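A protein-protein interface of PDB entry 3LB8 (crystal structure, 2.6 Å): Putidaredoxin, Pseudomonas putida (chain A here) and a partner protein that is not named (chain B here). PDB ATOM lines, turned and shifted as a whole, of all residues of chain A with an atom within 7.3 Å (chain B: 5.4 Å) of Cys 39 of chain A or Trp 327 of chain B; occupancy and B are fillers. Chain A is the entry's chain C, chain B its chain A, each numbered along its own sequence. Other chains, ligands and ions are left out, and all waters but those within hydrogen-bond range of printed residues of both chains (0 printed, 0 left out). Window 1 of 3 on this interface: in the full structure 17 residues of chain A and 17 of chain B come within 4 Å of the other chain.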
ATOM      1  N   MET A  24      -5.714  33.565   9.716  1.00  0.00           N
ATOM      2  CA  MET A  24      -5.322  32.364   8.988  1.00  0.00           C
ATOM      3  C   MET A  24      -4.283  32.691   7.922  1.00  0.00           C
ATOM      4  O   MET A  24      -3.205  32.097   7.898  1.00  0.00           O
ATOM      5  CB  MET A  24      -6.557  31.717   8.349  1.00  0.00           C
ATOM      6  CG  MET A  24      -6.275  30.551   7.395  1.00  0.00           C
ATOM      7  SD  MET A  24      -6.076  31.071   5.669  1.00  0.00           S
ATOM      8  CE  MET A  24      -4.373  30.779   5.405  1.00  0.00           C
ATOM      9  N   VAL A  36      -3.179  25.237   9.252  1.00  0.00           N
ATOM     10  CA  VAL A  36      -3.213  25.258   7.805  1.00  0.00           C
ATOM     11  C   VAL A  36      -4.569  25.802   7.366  1.00  0.00           C
ATOM     12  O   VAL A  36      -5.542  25.695   8.101  1.00  0.00           O
ATOM     13  CB  VAL A  36      -3.020  23.827   7.275  1.00  0.00           C
ATOM     14  CG1 VAL A  36      -1.754  23.227   7.879  1.00  0.00           C
ATOM     15  CG2 VAL A  36      -4.235  22.962   7.629  1.00  0.00           C
ATOM     16  N   GLY A  37      -4.638  26.390   6.178  1.00  0.00           N
ATOM     17  CA  GLY A  37      -5.904  26.929   5.700  1.00  0.00           C
ATOM     18  C   GLY A  37      -6.178  26.478   4.280  1.00  0.00           C
ATOM     19  O   GLY A  37      -6.369  27.291   3.376  1.00  0.00           O
ATOM     20  N   ASP A  38      -6.193  25.160   4.104  1.00  0.00           N
ATOM     21  CA  ASP A  38      -6.407  24.497   2.821  1.00  0.00           C
ATOM     22  C   ASP A  38      -7.366  25.150   1.833  1.00  0.00           C
ATOM     23  O   ASP A  38      -6.978  25.460   0.701  1.00  0.00           O
ATOM     24  CB  ASP A  38      -6.842  23.047   3.066  1.00  0.00           C
ATOM     25  CG  ASP A  38      -5.828  22.266   3.889  1.00  0.00           C
ATOM     26  OD1 ASP A  38      -6.075  21.074   4.182  1.00  0.00           O
ATOM     27  OD2 ASP A  38      -4.776  22.844   4.245  1.00  0.00           O
ATOM     28  N   CYS A  39      -8.607  25.373   2.255  1.00  0.00           N
ATOM     29  CA  CYS A  39      -9.611  25.950   1.366  1.00  0.00           C
ATOM     30  C   CYS A  39      -9.311  27.346   0.808  1.00  0.00           C
ATOM     31  O   CYS A  39      -9.844  27.730  -0.247  1.00  0.00           O
ATOM     32  CB  CYS A  39     -10.976  25.927   2.053  1.00  0.00           C
ATOM     33  SG  CYS A  39     -11.492  27.506   2.730  1.00  0.00           S
ATOM     34  N   GLY A  40      -8.458  28.101   1.496  1.00  0.00           N
ATOM     35  CA  GLY A  40      -8.102  29.428   1.011  1.00  0.00           C
ATOM     36  C   GLY A  40      -8.679  30.560   1.836  1.00  0.00           C
ATOM     37  O   GLY A  40      -8.462  31.732   1.538  1.00  0.00           O
ATOM     38  N   GLY A  41      -9.431  30.203   2.873  1.00  0.00           N
ATOM     39  CA  GLY A  41     -10.014  31.211   3.726  1.00  0.00           C
ATOM     40  C   GLY A  41     -11.394  31.649   3.289  1.00  0.00           C
ATOM     41  O   GLY A  41     -11.753  32.822   3.436  1.00  0.00           O
ATOM     42  N   SER A  42     -12.179  30.725   2.747  1.00  0.00           N
ATOM     43  CA  SER A  42     -13.523  31.076   2.315  1.00  0.00           C
ATOM     44  C   SER A  42     -14.538  30.442   3.258  1.00  0.00           C
ATOM     45  O   SER A  42     -15.742  30.578   3.066  1.00  0.00           O
ATOM     46  CB  SER A  42     -13.771  30.611   0.873  1.00  0.00           C
ATOM     47  OG  SER A  42     -13.917  29.204   0.781  1.00  0.00           O
ATOM     48  N   ALA A  43     -14.037  29.769   4.289  1.00  0.00           N
ATOM     49  CA  ALA A  43     -14.890  29.097   5.264  1.00  0.00           C
ATOM     50  C   ALA A  43     -15.569  27.933   4.563  1.00  0.00           C
ATOM     51  O   ALA A  43     -16.796  27.883   4.471  1.00  0.00           O
ATOM     52  CB  ALA A  43     -15.928  30.040   5.862  1.00  0.00           C
ATOM     53  N   SER A  44     -14.762  26.993   4.076  1.00  0.00           N
ATOM     54  CA  SER A  44     -15.284  25.832   3.377  1.00  0.00           C
ATOM     55  C   SER A  44     -14.603  24.521   3.789  1.00  0.00           C
ATOM     56  O   SER A  44     -15.010  23.440   3.369  1.00  0.00           O
ATOM     57  CB  SER A  44     -15.139  26.047   1.866  1.00  0.00           C
ATOM     58  OG  SER A  44     -15.651  27.308   1.489  1.00  0.00           O
ATOM     59  N   CYS A  45     -13.551  24.606   4.610  1.00  0.00           N
ATOM     60  CA  CYS A  45     -12.833  23.401   5.035  1.00  0.00           C
ATOM     61  C   CYS A  45     -12.658  23.198   6.552  1.00  0.00           C
ATOM     62  O   CYS A  45     -12.607  22.063   7.028  1.00  0.00           O
ATOM     63  CB  CYS A  45     -11.459  23.348   4.356  1.00  0.00           C
ATOM     64  SG  CYS A  45     -10.299  24.653   4.882  1.00  0.00           S
ATOM     65  N   ALA A  46     -12.551  24.287   7.303  1.00  0.00           N
ATOM     66  CA  ALA A  46     -12.423  24.202   8.770  1.00  0.00           C
ATOM     67  C   ALA A  46     -11.040  23.764   9.271  1.00  0.00           C
ATOM     68  O   ALA A  46     -10.919  23.208  10.368  1.00  0.00           O
ATOM     69  CB  ALA A  46     -13.481  23.266   9.309  1.00  0.00           C
ATOM     70  N   THR A  47      -9.999  23.998   8.471  1.00  0.00           N
ATOM     71  CA  THR A  47      -8.623  23.637   8.873  1.00  0.00           C
ATOM     72  C   THR A  47      -7.972  24.866   9.504  1.00  0.00           C
ATOM     73  O   THR A  47      -6.868  24.817  10.035  1.00  0.00           O
ATOM     74  CB  THR A  47      -7.789  23.160   7.672  1.00  0.00           C
ATOM     75  OG1 THR A  47      -7.810  24.159   6.657  1.00  0.00           O
ATOM     76  CG2 THR A  47      -8.346  21.862   7.111  1.00  0.00           C
ATOM     77  N   CYS A  48      -8.711  25.970   9.427  1.00  0.00           N
ATOM     78  CA  CYS A  48      -8.468  27.341  10.062  1.00  0.00           C
ATOM     79  C   CYS A  48      -8.727  27.407  11.460  1.00  0.00           C
ATOM     80  O   CYS A  48      -8.601  28.478  12.059  1.00  0.00           O
ATOM     81  CB  CYS A  48      -9.346  28.402   9.396  1.00  0.00           C
ATOM     82  SG  CYS A  48     -11.062  27.872   9.087  1.00  0.00           S
ATOM     83  N   ARG A  66     -22.742  29.857   8.444  1.00  0.00           N
ATOM     84  CA  ARG A  66     -21.737  29.257   7.574  1.00  0.00           C
ATOM     85  C   ARG A  66     -20.689  28.607   8.461  1.00  0.00           C
ATOM     86  O   ARG A  66     -20.491  27.389   8.429  1.00  0.00           O
ATOM     87  CB  ARG A  66     -21.063  30.337   6.727  1.00  0.00           C
ATOM     88  CG  ARG A  66     -21.199  30.168   5.227  1.00  0.00           C
ATOM     89  CD  ARG A  66     -19.913  29.696   4.566  1.00  0.00           C
ATOM     90  NE  ARG A  66     -19.755  30.345   3.265  1.00  0.00           N
ATOM     91  CZ  ARG A  66     -18.983  29.902   2.274  1.00  0.00           C
ATOM     92  NH1 ARG A  66     -18.277  28.790   2.409  1.00  0.00           N
ATOM     93  NH2 ARG A  66     -18.915  30.582   1.137  1.00  0.00           N
ATOM     94  N   CYS A  86      -9.872  32.156   9.651  1.00  0.00           N
ATOM     95  CA  CYS A  86      -9.991  32.742   8.318  1.00  0.00           C
ATOM     96  C   CYS A  86     -11.153  33.696   8.260  1.00  0.00           C
ATOM     97  O   CYS A  86     -11.186  34.566   7.395  1.00  0.00           O
ATOM     98  CB  CYS A  86     -10.104  31.693   7.212  1.00  0.00           C
ATOM     99  SG  CYS A  86     -11.497  30.566   7.507  1.00  0.00           S
ATOM    100  N   GLN A  87     -12.042  33.611   9.242  1.00  0.00           N
ATOM    101  CA  GLN A  87     -13.218  34.465   9.324  1.00  0.00           C
ATOM    102  C   GLN A  87     -13.010  35.500  10.405  1.00  0.00           C
ATOM    103  O   GLN A  87     -13.958  35.923  11.062  1.00  0.00           O
ATOM    104  CB  GLN A  87     -14.441  33.586   9.638  1.00  0.00           C
ATOM    105  CG  GLN A  87     -14.811  32.636   8.508  1.00  0.00           C
ATOM    106  CD  GLN A  87     -14.790  33.322   7.147  1.00  0.00           C
ATOM    107  OE1 GLN A  87     -15.583  34.229   6.873  1.00  0.00           O
ATOM    108  NE2 GLN A  87     -13.867  32.898   6.291  1.00  0.00           N
ATOM    109  N   SER B 300      -5.474  19.661  -8.330  1.00  0.00           N
ATOM    110  CA  SER B 300      -6.167  20.532  -7.398  1.00  0.00           C
ATOM    111  C   SER B 300      -5.341  20.891  -6.175  1.00  0.00           C
ATOM    112  O   SER B 300      -4.386  20.196  -5.827  1.00  0.00           O
ATOM    113  CB  SER B 300      -7.446  19.875  -6.924  1.00  0.00           C
ATOM    114  OG  SER B 300      -7.169  18.942  -5.897  1.00  0.00           O
ATOM    115  N   PRO B 302      -6.293  20.820  -2.876  1.00  0.00           N
ATOM    116  CA  PRO B 302      -6.380  19.834  -1.788  1.00  0.00           C
ATOM    117  C   PRO B 302      -5.527  18.596  -2.056  1.00  0.00           C
ATOM    118  O   PRO B 302      -4.889  18.051  -1.153  1.00  0.00           O
ATOM    119  CB  PRO B 302      -7.870  19.488  -1.732  1.00  0.00           C
ATOM    120  CG  PRO B 302      -8.545  20.696  -2.339  1.00  0.00           C
ATOM    121  CD  PRO B 302      -7.613  21.058  -3.479  1.00  0.00           C
ATOM    122  N   ASN B 303      -5.520  18.144  -3.306  1.00  0.00           N
ATOM    123  CA  ASN B 303      -4.761  16.963  -3.663  1.00  0.00           C
ATOM    124  C   ASN B 303      -3.267  17.208  -3.461  1.00  0.00           C
ATOM    125  O   ASN B 303      -2.551  16.309  -3.036  1.00  0.00           O
ATOM    126  CB  ASN B 303      -5.038  16.577  -5.118  1.00  0.00           C
ATOM    127  CG  ASN B 303      -4.184  15.410  -5.590  1.00  0.00           C
ATOM    128  OD1 ASN B 303      -4.406  14.263  -5.201  1.00  0.00           O
ATOM    129  ND2 ASN B 303      -3.184  15.706  -6.416  1.00  0.00           N
ATOM    130  N   ALA B 325     -11.155  12.344   0.731  1.00  0.00           N
ATOM    131  CA  ALA B 325     -12.023  12.629  -0.382  1.00  0.00           C
ATOM    132  C   ALA B 325     -11.353  13.750  -1.141  1.00  0.00           C
ATOM    133  O   ALA B 325     -10.932  14.738  -0.541  1.00  0.00           O
ATOM    134  CB  ALA B 325     -13.383  13.097   0.126  1.00  0.00           C
ATOM    135  N   PRO B 326     -11.191  13.597  -2.458  1.00  0.00           N
ATOM    136  CA  PRO B 326     -10.554  14.715  -3.151  1.00  0.00           C
ATOM    137  C   PRO B 326     -11.633  15.763  -3.358  1.00  0.00           C
ATOM    138  O   PRO B 326     -12.802  15.425  -3.471  1.00  0.00           O
ATOM    139  CB  PRO B 326     -10.091  14.102  -4.462  1.00  0.00           C
ATOM    140  CG  PRO B 326     -11.066  12.981  -4.682  1.00  0.00           C
ATOM    141  CD  PRO B 326     -11.254  12.396  -3.306  1.00  0.00           C
ATOM    142  N   TRP B 327     -11.271  17.036  -3.340  1.00  0.00           N
ATOM    143  CA  TRP B 327     -12.254  18.062  -3.588  1.00  0.00           C
ATOM    144  C   TRP B 327     -11.647  19.208  -4.373  1.00  0.00           C
ATOM    145  O   TRP B 327     -10.429  19.260  -4.582  1.00  0.00           O
ATOM    146  CB  TRP B 327     -12.920  18.545  -2.305  1.00  0.00           C
ATOM    147  CG  TRP B 327     -12.002  18.957  -1.207  1.00  0.00           C
ATOM    148  CD1 TRP B 327     -11.358  18.142  -0.335  1.00  0.00           C
ATOM    149  CD2 TRP B 327     -11.691  20.291  -0.819  1.00  0.00           C
ATOM    150  NE1 TRP B 327     -10.669  18.882   0.584  1.00  0.00           N
ATOM    151  CE2 TRP B 327     -10.856  20.209   0.313  1.00  0.00           C
ATOM    152  CE3 TRP B 327     -12.042  21.553  -1.317  1.00  0.00           C
ATOM    153  CZ2 TRP B 327     -10.355  21.350   0.971  1.00  0.00           C
ATOM    154  CZ3 TRP B 327     -11.541  22.695  -0.666  1.00  0.00           C
ATOM    155  CH2 TRP B 327     -10.709  22.579   0.465  1.00  0.00           C
ATOM    156  N   PHE B 328     -12.494  20.130  -4.801  1.00  0.00           N
ATOM    157  CA  PHE B 328     -12.058  21.217  -5.670  1.00  0.00           C
ATOM    158  C   PHE B 328     -13.157  22.272  -5.604  1.00  0.00           C
ATOM    159  O   PHE B 328     -14.259  21.983  -5.145  1.00  0.00           O
ATOM    160  CB  PHE B 328     -11.931  20.620  -7.105  1.00  0.00           C
ATOM    161  CG  PHE B 328     -11.700  21.630  -8.197  1.00  0.00           C
ATOM    162  CD1 PHE B 328     -12.776  22.225  -8.856  1.00  0.00           C
ATOM    163  CD2 PHE B 328     -10.388  22.010  -8.555  1.00  0.00           C
ATOM    164  CE1 PHE B 328     -12.560  23.191  -9.858  1.00  0.00           C
ATOM    165  CE2 PHE B 328     -10.150  22.972  -9.555  1.00  0.00           C
ATOM    166  CZ  PHE B 328     -11.234  23.568 -10.207  1.00  0.00           C
ATOM    167  N   TRP B 329     -12.881  23.487  -6.044  1.00  0.00           N
ATOM    168  CA  TRP B 329     -13.936  24.484  -6.026  1.00  0.00           C
ATOM    169  C   TRP B 329     -13.702  25.488  -7.140  1.00  0.00           C
ATOM    170  O   TRP B 329     -12.596  25.588  -7.663  1.00  0.00           O
ATOM    171  CB  TRP B 329     -13.997  25.202  -4.670  1.00  0.00           C
ATOM    172  CG  TRP B 329     -12.914  26.187  -4.489  1.00  0.00           C
ATOM    173  CD1 TRP B 329     -12.949  27.504  -4.820  1.00  0.00           C
ATOM    174  CD2 TRP B 329     -11.580  25.909  -4.056  1.00  0.00           C
ATOM    175  NE1 TRP B 329     -11.712  28.064  -4.629  1.00  0.00           N
ATOM    176  CE2 TRP B 329     -10.853  27.108  -4.159  1.00  0.00           C
ATOM    177  CE3 TRP B 329     -10.933  24.762  -3.588  1.00  0.00           C
ATOM    178  CZ2 TRP B 329      -9.504  27.198  -3.813  1.00  0.00           C
ATOM    179  CZ3 TRP B 329      -9.589  24.842  -3.240  1.00  0.00           C
ATOM    180  CH2 TRP B 329      -8.891  26.056  -3.354  1.00  0.00           C
ATOM    181  N   MET B 339     -16.867  20.875  -5.383  1.00  0.00           N
ATOM    182  CA  MET B 339     -17.042  19.499  -5.824  1.00  0.00           C
ATOM    183  C   MET B 339     -16.176  18.532  -5.045  1.00  0.00           C
ATOM    184  O   MET B 339     -14.958  18.680  -5.037  1.00  0.00           O
ATOM    185  CB  MET B 339     -16.675  19.369  -7.312  1.00  0.00           C
ATOM    186  CG  MET B 339     -17.473  20.229  -8.286  1.00  0.00           C
ATOM    187  SD  MET B 339     -17.001  22.004  -8.333  1.00  0.00           S
ATOM    188  CE  MET B 339     -18.655  22.780  -8.281  1.00  0.00           C
ATOM    189  N   VAL B 340     -16.779  17.542  -4.395  1.00  0.00           N
ATOM    190  CA  VAL B 340     -15.972  16.561  -3.670  1.00  0.00           C
ATOM    191  C   VAL B 340     -16.067  15.236  -4.422  1.00  0.00           C
ATOM    192  O   VAL B 340     -17.118  14.919  -4.982  1.00  0.00           O
ATOM    193  CB  VAL B 340     -16.446  16.361  -2.191  1.00  0.00           C
ATOM    194  CG1 VAL B 340     -17.902  15.951  -2.131  1.00  0.00           C
ATOM    195  CG2 VAL B 340     -15.613  15.308  -1.534  1.00  0.00           C
ATOM    196  N   GLY B 341     -14.969  14.483  -4.453  1.00  0.00           N
ATOM    197  CA  GLY B 341     -14.953  13.194  -5.132  1.00  0.00           C
ATOM    198  C   GLY B 341     -14.790  13.250  -6.642  1.00  0.00           C
ATOM    199  O   GLY B 341     -14.630  14.318  -7.228  1.00  0.00           O
ATOM    200  N   PHE B 382     -21.715  20.555   1.443  1.00  0.00           N
ATOM    201  CA  PHE B 382     -20.485  20.220   0.758  1.00  0.00           C
ATOM    202  C   PHE B 382     -19.459  19.646   1.731  1.00  0.00           C
ATOM    203  O   PHE B 382     -18.973  18.530   1.542  1.00  0.00           O
ATOM    204  CB  PHE B 382     -19.894  21.450   0.071  1.00  0.00           C
ATOM    205  CG  PHE B 382     -18.441  21.298  -0.268  1.00  0.00           C
ATOM    206  CD1 PHE B 382     -18.025  20.361  -1.210  1.00  0.00           C
ATOM    207  CD2 PHE B 382     -17.477  22.062   0.391  1.00  0.00           C
ATOM    208  CE1 PHE B 382     -16.671  20.180  -1.495  1.00  0.00           C
ATOM    209  CE2 PHE B 382     -16.122  21.893   0.115  1.00  0.00           C
ATOM    210  CZ  PHE B 382     -15.719  20.946  -0.831  1.00  0.00           C
ATOM    211  N   LYS B 386     -17.730  15.349   2.546  1.00  0.00           N
ATOM    212  CA  LYS B 386     -16.365  14.840   2.524  1.00  0.00           C
ATOM    213  C   LYS B 386     -16.260  13.585   3.380  1.00  0.00           C
ATOM    214  O   LYS B 386     -15.609  12.621   2.972  1.00  0.00           O
ATOM    215  CB  LYS B 386     -15.367  15.866   3.043  1.00  0.00           C
ATOM    216  CG  LYS B 386     -15.100  17.020   2.129  1.00  0.00           C
ATOM    217  CD  LYS B 386     -14.248  18.030   2.855  1.00  0.00           C
ATOM    218  CE  LYS B 386     -14.167  19.340   2.110  1.00  0.00           C
ATOM    219  NZ  LYS B 386     -13.472  20.370   2.952  1.00  0.00           N
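The side-chain amino group (NZ) of Lys 386 of chain B sits at hydrogen-bond distance from the backbone carbonyl oxygen (O) of Ser 44 of chain A, at 3.5 Å.
N of Gly 41 of chain A sits close to SG of Cys 39 of chain A, at 3.4 Å.
SG of Cys 39 of chain A lies close to N of Ser 42 of chain A, 3.3 Å away.
The backbone NH of Ala 43 of chain A sits close to the side-chain sulfur of Cys 39 of chain A (3.7 Å).
The side-chain sulfur (SG) of Cys 39 of chain A sits close to the backbone NH (N) of Ser 44 of chain A, 3.6 Å away.
The side-chain hydroxyl (OG) of Ser 44 of chain A is in hydrogen-bond range of the side-chain hydroxyl (OG) of Ser 42 of chain A.
The side-chain sulfur (SG) of Cys 45 of chain A lies close to the side-chain hydroxyl (OG1) of Thr 47 of chain A (3.1 Å).
Among the printed residues, merely in contact across the chains: Cys 39 of chain A with Trp 327 of chain B, Cys 39 of chain A with Trp 329 of chain B, Ser 44 of chain A with Phe 382 of chain B and Cys 45 of chain A with Lys 386 of chain B.
Of chain B, only Trp 327 (3.7 Å) and Trp 329 (3.6 Å) come within 4 Å of Cys 39 of chain A.
Trp 327 of chain B touches one residue of chain A.
Of the printed residues of chain A, Lys 386 of chain B touches Ser 44 (3.5 Å) and Cys 45 (3.7 Å).
Of the printed residues of chain A, Phe 382 of chain B touches Ser 44.
Of the printed residues of chain B, Cys 45 of chain A touches Lys 386.
Of the printed residues of chain A, Trp 329 of chain B touches Cys 39.
The nearest printed residue of chain B that does not touch Cys 39 of chain A is Lys 386 of chain B (6.2 Å).
The nearest printed residue of chain A that does not touch Phe 382 of chain B is Cys 45 of chain A (5.8 Å).
Of the 17 printed residues of chain A, 3 touch a printed residue of chain B.
Among the printed residues, no Asp or Glu carboxylate lies within 4 Å of a Lys or Arg side-chain nitrogen of the other chain.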
